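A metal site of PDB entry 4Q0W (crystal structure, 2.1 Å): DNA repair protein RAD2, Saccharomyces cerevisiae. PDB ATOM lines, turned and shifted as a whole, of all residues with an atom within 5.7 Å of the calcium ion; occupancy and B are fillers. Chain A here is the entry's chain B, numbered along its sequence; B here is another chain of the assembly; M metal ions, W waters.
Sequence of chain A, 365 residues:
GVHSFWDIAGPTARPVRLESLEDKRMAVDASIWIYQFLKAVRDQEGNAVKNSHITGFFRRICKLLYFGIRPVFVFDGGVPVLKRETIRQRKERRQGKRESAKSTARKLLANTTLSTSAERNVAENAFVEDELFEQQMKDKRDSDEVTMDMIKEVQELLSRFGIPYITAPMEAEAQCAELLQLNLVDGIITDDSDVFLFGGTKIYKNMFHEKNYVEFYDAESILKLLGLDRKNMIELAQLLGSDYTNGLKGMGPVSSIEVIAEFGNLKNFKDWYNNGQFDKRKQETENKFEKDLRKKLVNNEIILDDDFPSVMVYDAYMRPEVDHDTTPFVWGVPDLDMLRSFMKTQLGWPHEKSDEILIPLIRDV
N of Gly 1 lies close to OD2 of Asp 194, 3.2 Å away.
The side-chain carboxylate of Asp 192 lies close to the backbone NH of Gly 1, 3.0 Å away.
The side-chain carboxylate (OD2) of Asp 243 is in hydrogen-bond range of the backbone NH (N) of Gly 1 (2.9 Å).
Merely in contact with the calcium ion: Gly 1 (3.98 Å) and Asp 243 (3.7 Å).
Five residues have an atom within 4 Å of the calcium ion: Gly 1, Glu 173, Asp 192, Asp 194 and Asp 243.
The nearest printed residue that does not touch the calcium ion is Lys 83 (4.3 Å).
OD2 of Asp 194 binds the calcium ion.
Water W1 binds the calcium ion (2.5 Å).
The calcium ion is bound by OD2 of Asp 192 (2.5 Å).
OE1 of Glu 173 is bound to the calcium ion (2.6 Å).
Water W1 bridges OD2 of Asp 243 (2.8 Å) and OD1 of Asp 192 (3.4 Å).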
ATOM      1  N   GLY A   1     -12.684 -28.464 -16.368  1.00  0.00           N
ATOM      2  CA  GLY A   1     -11.615 -29.292 -15.857  1.00  0.00           C
ATOM      3  C   GLY A   1     -12.088 -30.634 -15.345  1.00  0.00           C
ATOM      4  O   GLY A   1     -13.280 -30.961 -15.376  1.00  0.00           O
ATOM      5  N   LYS A  83     -20.063 -31.971 -24.103  1.00  0.00           N
ATOM      6  CA  LYS A  83     -20.019 -30.989 -23.025  1.00  0.00           C
ATOM      7  C   LYS A  83     -21.397 -30.375 -22.798  1.00  0.00           C
ATOM      8  O   LYS A  83     -21.827 -30.218 -21.654  1.00  0.00           O
ATOM      9  CB  LYS A  83     -19.009 -29.882 -23.329  1.00  0.00           C
ATOM     10  CG  LYS A  83     -18.929 -28.828 -22.241  1.00  0.00           C
ATOM     11  CD  LYS A  83     -17.798 -27.844 -22.519  1.00  0.00           C
ATOM     12  CE  LYS A  83     -17.667 -26.850 -21.386  1.00  0.00           C
ATOM     13  NZ  LYS A  83     -16.509 -25.940 -21.593  1.00  0.00           N
ATOM     14  N   GLU A 173      -8.739 -24.490 -24.450  1.00  0.00           N
ATOM     15  CA  GLU A 173      -7.649 -25.270 -23.852  1.00  0.00           C
ATOM     16  C   GLU A 173      -7.130 -26.324 -24.820  1.00  0.00           C
ATOM     17  O   GLU A 173      -5.924 -26.600 -24.851  1.00  0.00           O
ATOM     18  CB  GLU A 173      -8.053 -25.993 -22.551  1.00  0.00           C
ATOM     19  CG  GLU A 173      -9.138 -25.316 -21.745  1.00  0.00           C
ATOM     20  CD  GLU A 173     -10.498 -25.746 -22.203  1.00  0.00           C
ATOM     21  OE1 GLU A 173     -10.854 -26.921 -21.943  1.00  0.00           O
ATOM     22  OE2 GLU A 173     -11.199 -24.923 -22.827  1.00  0.00           O
ATOM     23  N   ASP A 192      -7.300 -24.566 -16.032  1.00  0.00           N
ATOM     24  CA  ASP A 192      -8.268 -25.606 -16.391  1.00  0.00           C
ATOM     25  C   ASP A 192      -7.528 -26.921 -16.613  1.00  0.00           C
ATOM     26  O   ASP A 192      -6.801 -27.058 -17.591  1.00  0.00           O
ATOM     27  CB  ASP A 192      -8.975 -25.194 -17.681  1.00  0.00           C
ATOM     28  CG  ASP A 192     -10.115 -26.125 -18.059  1.00  0.00           C
ATOM     29  OD1 ASP A 192     -10.171 -27.263 -17.536  1.00  0.00           O
ATOM     30  OD2 ASP A 192     -10.939 -25.717 -18.910  1.00  0.00           O
ATOM     31  N   ASP A 194      -8.389 -29.637 -17.786  1.00  0.00           N
ATOM     32  CA  ASP A 194      -8.689 -30.293 -19.071  1.00  0.00           C
ATOM     33  C   ASP A 194      -7.486 -30.260 -20.026  1.00  0.00           C
ATOM     34  O   ASP A 194      -7.303 -31.159 -20.846  1.00  0.00           O
ATOM     35  CB  ASP A 194      -9.855 -29.601 -19.763  1.00  0.00           C
ATOM     36  CG  ASP A 194     -11.195 -30.141 -19.311  1.00  0.00           C
ATOM     37  OD1 ASP A 194     -11.250 -31.317 -18.878  1.00  0.00           O
ATOM     38  OD2 ASP A 194     -12.189 -29.390 -19.398  1.00  0.00           O
ATOM     39  N   PHE A 198      -6.094 -32.939 -23.057  1.00  0.00           N
ATOM     40  CA  PHE A 198      -6.008 -32.549 -24.457  1.00  0.00           C
ATOM     41  C   PHE A 198      -4.570 -32.623 -24.989  1.00  0.00           C
ATOM     42  O   PHE A 198      -4.279 -32.148 -26.100  1.00  0.00           O
ATOM     43  CB  PHE A 198      -6.562 -31.129 -24.657  1.00  0.00           C
ATOM     44  CG  PHE A 198      -8.067 -31.039 -24.572  1.00  0.00           C
ATOM     45  CD1 PHE A 198      -8.876 -31.905 -25.306  1.00  0.00           C
ATOM     46  CD2 PHE A 198      -8.679 -30.094 -23.753  1.00  0.00           C
ATOM     47  CE1 PHE A 198     -10.274 -31.809 -25.230  1.00  0.00           C
ATOM     48  CE2 PHE A 198     -10.064 -30.014 -23.664  1.00  0.00           C
ATOM     49  CZ  PHE A 198     -10.858 -30.874 -24.405  1.00  0.00           C
ATOM     50  N   ASP A 243     -16.261 -31.971 -17.710  1.00  0.00           N
ATOM     51  CA  ASP A 243     -17.251 -31.391 -18.616  1.00  0.00           C
ATOM     52  C   ASP A 243     -17.803 -32.404 -19.638  1.00  0.00           C
ATOM     53  O   ASP A 243     -18.795 -32.114 -20.311  1.00  0.00           O
ATOM     54  CB  ASP A 243     -16.650 -30.202 -19.377  1.00  0.00           C
ATOM     55  CG  ASP A 243     -16.001 -29.202 -18.449  1.00  0.00           C
ATOM     56  OD1 ASP A 243     -16.703 -28.261 -18.010  1.00  0.00           O
ATOM     57  OD2 ASP A 243     -14.792 -29.369 -18.142  1.00  0.00           O
ATOM     58  N   TYR A 244     -17.165 -33.568 -19.745  1.00  0.00           N
ATOM     59  CA  TYR A 244     -17.519 -34.535 -20.782  1.00  0.00           C
ATOM     60  C   TYR A 244     -18.051 -35.843 -20.208  1.00  0.00           C
ATOM     61  O   TYR A 244     -18.301 -36.800 -20.947  1.00  0.00           O
ATOM     62  CB  TYR A 244     -16.301 -34.801 -21.696  1.00  0.00           C
ATOM     63  CG  TYR A 244     -15.773 -33.568 -22.402  1.00  0.00           C
ATOM     64  CD1 TYR A 244     -15.146 -32.552 -21.701  1.00  0.00           C
ATOM     65  CD2 TYR A 244     -15.893 -33.420 -23.784  1.00  0.00           C
ATOM     66  CE1 TYR A 244     -14.672 -31.421 -22.332  1.00  0.00           C
ATOM     67  CE2 TYR A 244     -15.411 -32.287 -24.426  1.00  0.00           C
ATOM     68  CZ  TYR A 244     -14.808 -31.294 -23.693  1.00  0.00           C
ATOM     69  OH  TYR A 244     -14.319 -30.163 -24.307  1.00  0.00           O
ATOM     70  P    DA B   3     -16.618 -23.721 -16.375  1.00  0.00           P
ATOM     71  OP1  DA B   3     -16.680 -24.349 -17.721  1.00  0.00           O
ATOM     72  OP2  DA B   3     -17.610 -24.088 -15.333  1.00  0.00           O
ATOM     73  O5'  DA B   3     -15.163 -23.944 -15.737  1.00  0.00           O
ATOM     74  C5'  DA B   3     -14.493 -22.856 -15.132  1.00  0.00           C
ATOM     75  C4'  DA B   3     -13.849 -23.262 -13.812  1.00  0.00           C
ATOM     76  O4'  DA B   3     -14.267 -22.322 -12.794  1.00  0.00           O
ATOM     77  C3'  DA B   3     -14.288 -24.627 -13.292  1.00  0.00           C
ATOM     78  O3'  DA B   3     -13.306 -25.092 -12.363  1.00  0.00           O
ATOM     79  C2'  DA B   3     -15.591 -24.270 -12.589  1.00  0.00           C
ATOM     80  C1'  DA B   3     -15.172 -22.967 -11.906  1.00  0.00           C
ATOM     81  N9   DA B   3     -16.303 -22.077 -11.609  1.00  0.00           N
ATOM     82  C8   DA B   3     -17.601 -22.242 -11.985  1.00  0.00           C
ATOM     83  N7   DA B   3     -18.402 -21.283 -11.569  1.00  0.00           N
ATOM     84  C5   DA B   3     -17.562 -20.452 -10.855  1.00  0.00           C
ATOM     85  C6   DA B   3     -17.803 -19.247 -10.152  1.00  0.00           C
ATOM     86  N6   DA B   3     -19.001 -18.669 -10.066  1.00  0.00           N
ATOM     87  N1   DA B   3     -16.738 -18.668  -9.545  1.00  0.00           N
ATOM     88  C2   DA B   3     -15.527 -19.258  -9.643  1.00  0.00           C
ATOM     89  N3   DA B   3     -15.182 -20.379 -10.269  1.00  0.00           N
ATOM     90  C4   DA B   3     -16.258 -20.931 -10.861  1.00  0.00           C
HETATM   91 CA    CA M   1     -12.658 -27.073 -20.102  1.00  0.00          CA
HETATM   92  O   HOH W   1     -13.552 -26.859 -17.809  1.00  0.00           O
